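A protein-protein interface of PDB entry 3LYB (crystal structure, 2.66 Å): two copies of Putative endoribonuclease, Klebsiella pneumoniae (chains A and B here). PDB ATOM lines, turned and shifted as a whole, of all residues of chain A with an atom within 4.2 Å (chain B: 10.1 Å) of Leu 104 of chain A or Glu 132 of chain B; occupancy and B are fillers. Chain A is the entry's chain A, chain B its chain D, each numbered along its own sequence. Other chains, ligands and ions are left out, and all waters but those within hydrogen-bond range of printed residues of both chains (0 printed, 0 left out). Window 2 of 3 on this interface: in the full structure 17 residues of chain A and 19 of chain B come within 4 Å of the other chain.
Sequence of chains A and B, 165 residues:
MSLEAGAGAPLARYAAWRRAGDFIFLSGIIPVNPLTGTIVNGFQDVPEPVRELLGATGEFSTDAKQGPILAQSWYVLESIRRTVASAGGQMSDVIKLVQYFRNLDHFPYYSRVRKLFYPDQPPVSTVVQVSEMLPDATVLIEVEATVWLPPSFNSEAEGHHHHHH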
ATOM      1  N   PHE A 101       3.630  -8.828  -8.572  1.00  0.00           N
ATOM      2  CA  PHE A 101       4.059  -8.139  -7.363  1.00  0.00           C
ATOM      3  C   PHE A 101       3.571  -8.897  -6.157  1.00  0.00           C
ATOM      4  O   PHE A 101       2.512  -9.550  -6.229  1.00  0.00           O
ATOM      5  CB  PHE A 101       3.394  -6.788  -7.318  1.00  0.00           C
ATOM      6  CG  PHE A 101       3.925  -5.825  -8.320  1.00  0.00           C
ATOM      7  CD1 PHE A 101       3.523  -5.896  -9.647  1.00  0.00           C
ATOM      8  CD2 PHE A 101       4.807  -4.823  -7.929  1.00  0.00           C
ATOM      9  CE1 PHE A 101       4.040  -4.987 -10.579  1.00  0.00           C
ATOM     10  CE2 PHE A 101       5.297  -3.926  -8.828  1.00  0.00           C
ATOM     11  CZ  PHE A 101       4.924  -3.991 -10.156  1.00  0.00           C
ATOM     12  N   ASN A 103       3.275  -6.929  -3.395  1.00  0.00           N
ATOM     13  CA  ASN A 103       2.563  -5.801  -2.853  1.00  0.00           C
ATOM     14  C   ASN A 103       2.365  -4.692  -3.915  1.00  0.00           C
ATOM     15  O   ASN A 103       3.309  -3.977  -4.283  1.00  0.00           O
ATOM     16  CB  ASN A 103       3.342  -5.262  -1.647  1.00  0.00           C
ATOM     17  CG  ASN A 103       2.513  -4.327  -0.785  1.00  0.00           C
ATOM     18  OD1 ASN A 103       1.547  -3.705  -1.236  1.00  0.00           O
ATOM     19  ND2 ASN A 103       2.879  -4.240   0.464  1.00  0.00           N
ATOM     20  N   LEU A 104       1.133  -4.531  -4.387  1.00  0.00           N
ATOM     21  CA  LEU A 104       0.884  -3.529  -5.390  1.00  0.00           C
ATOM     22  C   LEU A 104       1.281  -2.134  -4.928  1.00  0.00           C
ATOM     23  O   LEU A 104       1.518  -1.241  -5.747  1.00  0.00           O
ATOM     24  CB  LEU A 104      -0.541  -3.589  -5.925  1.00  0.00           C
ATOM     25  CG  LEU A 104      -0.607  -4.636  -7.054  1.00  0.00           C
ATOM     26  CD1 LEU A 104      -1.975  -4.720  -7.671  1.00  0.00           C
ATOM     27  CD2 LEU A 104       0.426  -4.430  -8.138  1.00  0.00           C
ATOM     28  N   ASP A 105       1.406  -1.940  -3.623  1.00  0.00           N
ATOM     29  CA  ASP A 105       1.896  -0.637  -3.140  1.00  0.00           C
ATOM     30  C   ASP A 105       3.313  -0.325  -3.661  1.00  0.00           C
ATOM     31  O   ASP A 105       3.777   0.802  -3.563  1.00  0.00           O
ATOM     32  CB  ASP A 105       1.804  -0.532  -1.609  1.00  0.00           C
ATOM     33  CG  ASP A 105       0.358  -0.587  -1.114  1.00  0.00           C
ATOM     34  OD1 ASP A 105      -0.574  -0.349  -1.923  1.00  0.00           O
ATOM     35  OD2 ASP A 105       0.144  -0.894   0.072  1.00  0.00           O
ATOM     36  N   HIS A 106       3.980  -1.315  -4.242  1.00  0.00           N
ATOM     37  CA  HIS A 106       5.293  -1.103  -4.793  1.00  0.00           C
ATOM     38  C   HIS A 106       5.209  -0.626  -6.226  1.00  0.00           C
ATOM     39  O   HIS A 106       6.225  -0.244  -6.811  1.00  0.00           O
ATOM     40  CB  HIS A 106       6.091  -2.396  -4.758  1.00  0.00           C
ATOM     41  CG  HIS A 106       6.534  -2.791  -3.395  1.00  0.00           C
ATOM     42  ND1 HIS A 106       6.514  -4.095  -2.959  1.00  0.00           N
ATOM     43  CD2 HIS A 106       7.006  -2.055  -2.362  1.00  0.00           C
ATOM     44  CE1 HIS A 106       6.982  -4.151  -1.725  1.00  0.00           C
ATOM     45  NE2 HIS A 106       7.298  -2.926  -1.345  1.00  0.00           N
ATOM     46  N   PHE A 107       4.008  -0.673  -6.803  1.00  0.00           N
ATOM     47  CA  PHE A 107       3.825  -0.269  -8.196  1.00  0.00           C
ATOM     48  C   PHE A 107       4.443   1.110  -8.567  1.00  0.00           C
ATOM     49  O   PHE A 107       5.203   1.186  -9.527  1.00  0.00           O
ATOM     50  CB  PHE A 107       2.364  -0.350  -8.656  1.00  0.00           C
ATOM     51  CG  PHE A 107       2.189   0.043 -10.088  1.00  0.00           C
ATOM     52  CD1 PHE A 107       2.533  -0.850 -11.110  1.00  0.00           C
ATOM     53  CD2 PHE A 107       1.756   1.331 -10.422  1.00  0.00           C
ATOM     54  CE1 PHE A 107       2.414  -0.490 -12.436  1.00  0.00           C
ATOM     55  CE2 PHE A 107       1.635   1.718 -11.767  1.00  0.00           C
ATOM     56  CZ  PHE A 107       1.971   0.812 -12.780  1.00  0.00           C
ATOM     57  N   PRO A 108       4.139   2.189  -7.802  1.00  0.00           N
ATOM     58  CA  PRO A 108       4.740   3.491  -8.160  1.00  0.00           C
ATOM     59  C   PRO A 108       6.259   3.419  -8.291  1.00  0.00           C
ATOM     60  O   PRO A 108       6.834   4.038  -9.198  1.00  0.00           O
ATOM     61  CB  PRO A 108       4.352   4.391  -7.001  1.00  0.00           C
ATOM     62  CG  PRO A 108       3.090   3.764  -6.489  1.00  0.00           C
ATOM     63  CD  PRO A 108       3.325   2.300  -6.578  1.00  0.00           C
ATOM     64  N   VAL A 127      -0.635  -6.288 -14.813  1.00  0.00           N
ATOM     65  CA  VAL A 127      -0.065  -6.126 -13.495  1.00  0.00           C
ATOM     66  C   VAL A 127      -0.990  -6.769 -12.462  1.00  0.00           C
ATOM     67  O   VAL A 127      -2.172  -6.407 -12.348  1.00  0.00           O
ATOM     68  CB  VAL A 127       0.023  -4.635 -13.150  1.00  0.00           C
ATOM     69  CG1 VAL A 127       0.318  -4.436 -11.667  1.00  0.00           C
ATOM     70  CG2 VAL A 127       1.057  -3.918 -14.047  1.00  0.00           C
ATOM     71  N   VAL A 128      -0.450  -7.708 -11.696  1.00  0.00           N
ATOM     72  CA  VAL A 128      -1.207  -8.351 -10.632  1.00  0.00           C
ATOM     73  C   VAL A 128      -0.388  -8.523  -9.381  1.00  0.00           C
ATOM     74  O   VAL A 128       0.841  -8.601  -9.435  1.00  0.00           O
ATOM     75  CB  VAL A 128      -1.713  -9.750 -11.020  1.00  0.00           C
ATOM     76  CG1 VAL A 128      -2.795  -9.650 -12.086  1.00  0.00           C
ATOM     77  CG2 VAL A 128      -0.579 -10.617 -11.493  1.00  0.00           C
ATOM     78  N   GLN A 129      -1.096  -8.590  -8.258  1.00  0.00           N
ATOM     79  CA  GLN A 129      -0.509  -8.992  -7.001  1.00  0.00           C
ATOM     80  C   GLN A 129      -0.776 -10.462  -6.814  1.00  0.00           C
ATOM     81  O   GLN A 129      -1.923 -10.894  -6.803  1.00  0.00           O
ATOM     82  CB  GLN A 129      -1.112  -8.204  -5.845  1.00  0.00           C
ATOM     83  CG  GLN A 129      -0.295  -8.290  -4.557  1.00  0.00           C
ATOM     84  CD  GLN A 129      -0.860  -7.409  -3.459  1.00  0.00           C
ATOM     85  OE1 GLN A 129      -0.871  -6.176  -3.575  1.00  0.00           O
ATOM     86  NE2 GLN A 129      -1.370  -8.034  -2.409  1.00  0.00           N
ATOM     87  N   ILE B  30      -9.222  -3.220 -16.659  1.00  0.00           N
ATOM     88  CA  ILE B  30      -9.973  -3.183 -15.410  1.00  0.00           C
ATOM     89  C   ILE B  30     -11.214  -2.289 -15.534  1.00  0.00           C
ATOM     90  O   ILE B  30     -11.289  -1.496 -16.449  1.00  0.00           O
ATOM     91  CB  ILE B  30      -9.058  -2.807 -14.199  1.00  0.00           C
ATOM     92  CG1 ILE B  30      -8.175  -1.604 -14.514  1.00  0.00           C
ATOM     93  CG2 ILE B  30      -8.130  -3.961 -13.859  1.00  0.00           C
ATOM     94  CD1 ILE B  30      -8.632  -0.335 -13.908  1.00  0.00           C
ATOM     95  N   ILE B  39     -14.323   3.658 -10.174  1.00  0.00           N
ATOM     96  CA  ILE B  39     -14.298   2.222 -10.366  1.00  0.00           C
ATOM     97  C   ILE B  39     -15.709   1.694 -10.333  1.00  0.00           C
ATOM     98  O   ILE B  39     -16.421   1.849  -9.342  1.00  0.00           O
ATOM     99  CB  ILE B  39     -13.441   1.532  -9.284  1.00  0.00           C
ATOM    100  CG1 ILE B  39     -11.963   1.606  -9.678  1.00  0.00           C
ATOM    101  CG2 ILE B  39     -13.858   0.073  -9.068  1.00  0.00           C
ATOM    102  CD1 ILE B  39     -11.072   1.730  -8.497  1.00  0.00           C
ATOM    103  N   TYR B 100      -8.106 -12.716 -14.327  1.00  0.00           N
ATOM    104  CA  TYR B 100      -7.704 -12.624 -12.925  1.00  0.00           C
ATOM    105  C   TYR B 100      -8.894 -12.254 -12.026  1.00  0.00           C
ATOM    106  O   TYR B 100      -9.641 -11.334 -12.334  1.00  0.00           O
ATOM    107  CB  TYR B 100      -6.552 -11.605 -12.782  1.00  0.00           C
ATOM    108  CG  TYR B 100      -5.343 -11.880 -13.678  1.00  0.00           C
ATOM    109  CD1 TYR B 100      -4.400 -12.860 -13.349  1.00  0.00           C
ATOM    110  CD2 TYR B 100      -5.147 -11.169 -14.864  1.00  0.00           C
ATOM    111  CE1 TYR B 100      -3.287 -13.118 -14.175  1.00  0.00           C
ATOM    112  CE2 TYR B 100      -4.033 -11.426 -15.712  1.00  0.00           C
ATOM    113  CZ  TYR B 100      -3.115 -12.395 -15.351  1.00  0.00           C
ATOM    114  OH  TYR B 100      -2.036 -12.648 -16.171  1.00  0.00           O
ATOM    115  N   PHE B 101      -9.067 -12.980 -10.921  1.00  0.00           N
ATOM    116  CA  PHE B 101     -10.123 -12.696  -9.927  1.00  0.00           C
ATOM    117  C   PHE B 101      -9.553 -12.449  -8.536  1.00  0.00           C
ATOM    118  O   PHE B 101      -8.528 -13.062  -8.154  1.00  0.00           O
ATOM    119  CB  PHE B 101     -11.073 -13.890  -9.797  1.00  0.00           C
ATOM    120  CG  PHE B 101     -11.938 -14.138 -11.008  1.00  0.00           C
ATOM    121  CD1 PHE B 101     -11.431 -14.825 -12.119  1.00  0.00           C
ATOM    122  CD2 PHE B 101     -13.268 -13.717 -11.023  1.00  0.00           C
ATOM    123  CE1 PHE B 101     -12.226 -15.068 -13.248  1.00  0.00           C
ATOM    124  CE2 PHE B 101     -14.095 -13.962 -12.156  1.00  0.00           C
ATOM    125  CZ  PHE B 101     -13.565 -14.633 -13.270  1.00  0.00           C
ATOM    126  N   ARG B 102     -10.222 -11.597  -7.763  1.00  0.00           N
ATOM    127  CA  ARG B 102      -9.990 -11.552  -6.315  1.00  0.00           C
ATOM    128  C   ARG B 102     -10.672 -12.742  -5.649  1.00  0.00           C
ATOM    129  O   ARG B 102     -10.264 -13.193  -4.580  1.00  0.00           O
ATOM    130  CB  ARG B 102     -10.500 -10.255  -5.665  1.00  0.00           C
ATOM    131  CG  ARG B 102      -9.676  -9.044  -5.999  1.00  0.00           C
ATOM    132  CD  ARG B 102      -9.675  -7.967  -4.937  1.00  0.00           C
ATOM    133  NE  ARG B 102      -9.035  -8.466  -3.747  1.00  0.00           N
ATOM    134  CZ  ARG B 102      -9.588  -8.425  -2.548  1.00  0.00           C
ATOM    135  NH1 ARG B 102     -10.768  -7.838  -2.410  1.00  0.00           N
ATOM    136  NH2 ARG B 102      -8.958  -8.950  -1.490  1.00  0.00           N
ATOM    137  N   ASN B 103     -11.727 -13.252  -6.281  1.00  0.00           N
ATOM    138  CA  ASN B 103     -12.509 -14.310  -5.664  1.00  0.00           C
ATOM    139  C   ASN B 103     -13.170 -15.185  -6.686  1.00  0.00           C
ATOM    140  O   ASN B 103     -14.200 -14.831  -7.223  1.00  0.00           O
ATOM    141  CB  ASN B 103     -13.569 -13.686  -4.766  1.00  0.00           C
ATOM    142  CG  ASN B 103     -14.245 -14.698  -3.886  1.00  0.00           C
ATOM    143  OD1 ASN B 103     -14.287 -15.892  -4.196  1.00  0.00           O
ATOM    144  ND2 ASN B 103     -14.769 -14.234  -2.767  1.00  0.00           N
ATOM    145  N   VAL B 128      -7.437 -17.562 -12.864  1.00  0.00           N
ATOM    146  CA  VAL B 128      -6.741 -17.675 -11.586  1.00  0.00           C
ATOM    147  C   VAL B 128      -7.268 -16.652 -10.601  1.00  0.00           C
ATOM    148  O   VAL B 128      -7.689 -15.559 -10.997  1.00  0.00           O
ATOM    149  CB  VAL B 128      -5.175 -17.494 -11.705  1.00  0.00           C
ATOM    150  CG1 VAL B 128      -4.570 -18.618 -12.488  1.00  0.00           C
ATOM    151  CG2 VAL B 128      -4.804 -16.171 -12.334  1.00  0.00           C
ATOM    152  N   GLN B 129      -7.230 -17.020  -9.320  1.00  0.00           N
ATOM    153  CA  GLN B 129      -7.482 -16.087  -8.237  1.00  0.00           C
ATOM    154  C   GLN B 129      -6.151 -15.506  -7.780  1.00  0.00           C
ATOM    155  O   GLN B 129      -5.206 -16.244  -7.449  1.00  0.00           O
ATOM    156  CB  GLN B 129      -8.204 -16.758  -7.056  1.00  0.00           C
ATOM    157  CG  GLN B 129      -8.735 -15.769  -5.991  1.00  0.00           C
ATOM    158  CD  GLN B 129      -9.502 -16.453  -4.853  1.00  0.00           C
ATOM    159  OE1 GLN B 129     -10.553 -17.061  -5.071  1.00  0.00           O
ATOM    160  NE2 GLN B 129      -8.988 -16.338  -3.638  1.00  0.00           N
ATOM    161  N   VAL B 130      -6.082 -14.182  -7.784  1.00  0.00           N
ATOM    162  CA  VAL B 130      -4.892 -13.475  -7.328  1.00  0.00           C
ATOM    163  C   VAL B 130      -5.277 -12.654  -6.112  1.00  0.00           C
ATOM    164  O   VAL B 130      -6.385 -12.772  -5.644  1.00  0.00           O
ATOM    165  CB  VAL B 130      -4.259 -12.626  -8.469  1.00  0.00           C
ATOM    166  CG1 VAL B 130      -4.015 -13.527  -9.669  1.00  0.00           C
ATOM    167  CG2 VAL B 130      -5.146 -11.420  -8.867  1.00  0.00           C
ATOM    168  N   SER B 131      -4.385 -11.807  -5.612  1.00  0.00           N
ATOM    169  CA  SER B 131      -4.682 -11.085  -4.374  1.00  0.00           C
ATOM    170  C   SER B 131      -5.417  -9.817  -4.615  1.00  0.00           C
ATOM    171  O   SER B 131      -6.382  -9.504  -3.944  1.00  0.00           O
ATOM    172  CB  SER B 131      -3.413 -10.788  -3.621  1.00  0.00           C
ATOM    173  OG  SER B 131      -2.902 -12.009  -3.144  1.00  0.00           O
ATOM    174  N   GLU B 132      -4.932  -9.073  -5.588  1.00  0.00           N
ATOM    175  CA  GLU B 132      -5.348  -7.707  -5.765  1.00  0.00           C
ATOM    176  C   GLU B 132      -4.939  -7.383  -7.179  1.00  0.00           C
ATOM    177  O   GLU B 132      -4.043  -8.026  -7.737  1.00  0.00           O
ATOM    178  CB  GLU B 132      -4.580  -6.788  -4.778  1.00  0.00           C
ATOM    179  CG  GLU B 132      -5.469  -5.847  -4.029  1.00  0.00           C
ATOM    180  CD  GLU B 132      -4.741  -4.870  -3.166  1.00  0.00           C
ATOM    181  OE1 GLU B 132      -4.424  -5.188  -1.991  1.00  0.00           O
ATOM    182  OE2 GLU B 132      -4.516  -3.747  -3.662  1.00  0.00           O
ATOM    183  N   MET B 133      -5.607  -6.393  -7.756  1.00  0.00           N
ATOM    184  CA  MET B 133      -5.078  -5.730  -8.933  1.00  0.00           C
ATOM    185  C   MET B 133      -5.114  -4.197  -8.789  1.00  0.00           C
ATOM    186  O   MET B 133      -5.540  -3.675  -7.754  1.00  0.00           O
ATOM    187  CB  MET B 133      -5.680  -6.265 -10.246  1.00  0.00           C
ATOM    188  CG  MET B 133      -7.064  -6.775 -10.179  1.00  0.00           C
ATOM    189  SD  MET B 133      -7.289  -8.696  -9.788  1.00  0.00           S
ATOM    190  CE  MET B 133      -9.166  -8.714 -10.154  1.00  0.00           C
ATOM    191  N   LEU B 134      -4.601  -3.489  -9.789  1.00  0.00           N
ATOM    192  CA  LEU B 134      -4.625  -2.037  -9.797  1.00  0.00           C
ATOM    193  C   LEU B 134      -6.032  -1.535 -10.093  1.00  0.00           C
ATOM    194  O   LEU B 134      -6.766  -2.172 -10.840  1.00  0.00           O
ATOM    195  CB  LEU B 134      -3.674  -1.507 -10.867  1.00  0.00           C
ATOM    196  CG  LEU B 134      -2.211  -1.651 -10.477  1.00  0.00           C
ATOM    197  CD1 LEU B 134      -1.309  -1.297 -11.667  1.00  0.00           C
ATOM    198  CD2 LEU B 134      -1.903  -0.807  -9.224  1.00  0.00           C
ATOM    199  N   PRO B 135      -6.403  -0.362  -9.546  1.00  0.00           N
ATOM    200  CA  PRO B 135      -5.657   0.505  -8.624  1.00  0.00           C
ATOM    201  C   PRO B 135      -5.937   0.287  -7.138  1.00  0.00           C
ATOM    202  O   PRO B 135      -5.334   0.950  -6.306  1.00  0.00           O
ATOM    203  CB  PRO B 135      -6.176   1.882  -9.004  1.00  0.00           C
ATOM    204  CG  PRO B 135      -7.610   1.594  -9.360  1.00  0.00           C
ATOM    205  CD  PRO B 135      -7.547   0.352 -10.149  1.00  0.00           C
ATOM    206  N   ASP B 136      -6.888  -0.579  -6.804  1.00  0.00           N
ATOM    207  CA  ASP B 136      -7.165  -0.937  -5.406  1.00  0.00           C
ATOM    208  C   ASP B 136      -8.072  -2.156  -5.340  1.00  0.00           C
ATOM    209  O   ASP B 136      -8.481  -2.701  -6.381  1.00  0.00           O
ATOM    210  CB  ASP B 136      -7.795   0.223  -4.629  1.00  0.00           C
ATOM    211  CG  ASP B 136      -9.153   0.648  -5.198  1.00  0.00           C
ATOM    212  OD1 ASP B 136      -9.923  -0.241  -5.663  1.00  0.00           O
ATOM    213  OD2 ASP B 136      -9.454   1.875  -5.178  1.00  0.00           O
ATOM    214  N   ALA B 137      -8.406  -2.549  -4.114  1.00  0.00           N
ATOM    215  CA  ALA B 137      -8.962  -3.854  -3.839  1.00  0.00           C
ATOM    216  C   ALA B 137     -10.401  -4.048  -4.325  1.00  0.00           C
ATOM    217  O   ALA B 137     -10.898  -5.174  -4.366  1.00  0.00           O
ATOM    218  CB  ALA B 137      -8.848  -4.159  -2.337  1.00  0.00           C
ATOM    219  N   THR B 138     -11.068  -2.963  -4.694  1.00  0.00           N
ATOM    220  CA  THR B 138     -12.453  -3.052  -5.166  1.00  0.00           C
ATOM    221  C   THR B 138     -12.561  -3.590  -6.601  1.00  0.00           C
ATOM    222  O   THR B 138     -13.670  -3.952  -7.036  1.00  0.00           O
ATOM    223  CB  THR B 138     -13.179  -1.694  -5.105  1.00  0.00           C
ATOM    224  OG1 THR B 138     -12.571  -0.783  -6.035  1.00  0.00           O
ATOM    225  CG2 THR B 138     -13.117  -1.103  -3.684  1.00  0.00           C
ATOM    226  N   VAL B 139     -11.438  -3.644  -7.328  1.00  0.00           N
ATOM    227  CA  VAL B 139     -11.411  -4.330  -8.610  1.00  0.00           C
ATOM    228  C   VAL B 139     -11.502  -5.809  -8.327  1.00  0.00           C
ATOM    229  O   VAL B 139     -10.716  -6.331  -7.551  1.00  0.00           O
ATOM    230  CB  VAL B 139     -10.151  -4.017  -9.429  1.00  0.00           C
ATOM    231  CG1 VAL B 139     -10.043  -4.941 -10.608  1.00  0.00           C
ATOM    232  CG2 VAL B 139     -10.172  -2.556  -9.903  1.00  0.00           C
ATOM    233  N   LEU B 140     -12.478  -6.468  -8.957  1.00  0.00           N
ATOM    234  CA  LEU B 140     -12.789  -7.881  -8.725  1.00  0.00           C
ATOM    235  C   LEU B 140     -12.421  -8.770  -9.903  1.00  0.00           C
ATOM    236  O   LEU B 140     -12.402 -10.000  -9.796  1.00  0.00           O
ATOM    237  CB  LEU B 140     -14.272  -8.032  -8.430  1.00  0.00           C
ATOM    238  CG  LEU B 140     -14.768  -7.302  -7.182  1.00  0.00           C
ATOM    239  CD1 LEU B 140     -16.281  -7.450  -7.076  1.00  0.00           C
ATOM    240  CD2 LEU B 140     -14.127  -7.828  -5.912  1.00  0.00           C
ATOM    241  N   ILE B 141     -12.112  -8.141 -11.027  1.00  0.00           N
ATOM    242  CA  ILE B 141     -11.881  -8.851 -12.260  1.00  0.00           C
ATOM    243  C   ILE B 141     -10.967  -7.992 -13.153  1.00  0.00           C
ATOM    244  O   ILE B 141     -11.117  -6.766 -13.242  1.00  0.00           O
ATOM    245  CB  ILE B 141     -13.230  -9.218 -12.947  1.00  0.00           C
ATOM    246  CG1 ILE B 141     -13.020  -9.875 -14.317  1.00  0.00           C
ATOM    247  CG2 ILE B 141     -14.140  -7.986 -13.097  1.00  0.00           C
ATOM    248  CD1 ILE B 141     -12.540 -11.301 -14.286  1.00  0.00           C
ATOM    249  N   GLU B 142      -9.969  -8.638 -13.747  1.00  0.00           N
ATOM    250  CA  GLU B 142      -9.141  -8.030 -14.769  1.00  0.00           C
ATOM    251  C   GLU B 142      -8.978  -9.087 -15.856  1.00  0.00           C
ATOM    252  O   GLU B 142      -8.709 -10.259 -15.554  1.00  0.00           O
ATOM    253  CB  GLU B 142      -7.794  -7.585 -14.211  1.00  0.00           C
ATOM    254  CG  GLU B 142      -6.932  -6.857 -15.268  1.00  0.00           C
ATOM    255  CD  GLU B 142      -5.559  -6.443 -14.767  1.00  0.00           C
ATOM    256  OE1 GLU B 142      -5.352  -6.438 -13.533  1.00  0.00           O
ATOM    257  OE2 GLU B 142      -4.674  -6.108 -15.595  1.00  0.00           O
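Printed residues of chain B within 4 Å of Leu 104 of chain A: Glu 132, Met 133 and Leu 134.
No residue of chain B comes within 4 Å of Asp 105 of chain A.
Printed residues of chain B within 4 Å of Phe 107 of chain A: Leu 134 (3.9 Å).
Of the printed residues of chain B, Val 127 of chain A touches Leu 134 (3.5 Å) and Glu 142 (3.4 Å).
Of chain B, only Tyr 100 (3.7 Å) comes within 4 Å of Val 128 of chain A.
Gln 129 of chain A touches three residues of chain B.
Asn 103 of chain B touches none of the printed residues of chain A.
Printed residues of chain A within 4 Å of Ser 131 of chain B: Gln 129.
Of chain A, only Leu 104 and Gln 129 come within 4 Å of Glu 132 of chain B.
Of the printed residues of chain A, Glu 142 of chain B touches Val 127 (3.4 Å).
The nearest printed residue of chain A that does not touch Leu 134 of chain B is Val 128 of chain A (6.0 Å).
4 positions are printed for both chains.
The backbone NH of Ser 131 of chain B sits at hydrogen-bond distance from the backbone carbonyl oxygen of Gln 129 of chain A, at 2.9 Å.
O of Glu 132 of chain B is in hydrogen-bond range of N of Gln 129 of chain A.
The side-chain carboxylate (OE1) of Glu 142 of chain B sits close to the backbone carbonyl oxygen (O) of Val 127 of chain A, 3.4 Å away.
Printed residues of chain A that touch a printed residue of chain B: Leu 104, Phe 107, Val 127, Val 128 and Gln 129.
Printed residues of chain B that touch a printed residue of chain A: Tyr 100, Val 130, Ser 131, Glu 132, Met 133, Leu 134 and Glu 142.
The backbone NH (N) of Phe 101 of chain A sits at hydrogen-bond distance from the backbone carbonyl oxygen (O) of Val 128 of chain A (2.9 Å).
The side-chain amide oxygen of Gln 129 of chain A lies within hydrogen-bond range of the backbone NH of Leu 104 of chain A (2.7 Å).
N of Tyr 100 of chain B is in hydrogen-bond range of O of Glu 142 of chain B (2.8 Å).
The backbone carbonyl oxygen (O) of Phe 101 of chain B lies within hydrogen-bond range of the backbone NH (N) of Val 130 of chain B, at 2.7 Å.
The guanidinium group (NE) of Arg 102 of chain B sits at hydrogen-bond distance from the backbone carbonyl oxygen (O) of Ser 131 of chain B (2.9 Å).
Among the printed residues, merely in contact across the chains: Gln 129 of chain A with Val 130 of chain B, Leu 104 of chain A with Met 133 of chain B, Val 127 of chain A with Leu 134 of chain B, Leu 104 of chain A with Leu 134 of chain B, Val 128 of chain A with Tyr 100 of chain B, Phe 107 of chain A with Leu 134 of chain B and Leu 104 of chain A with Glu 132 of chain B.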
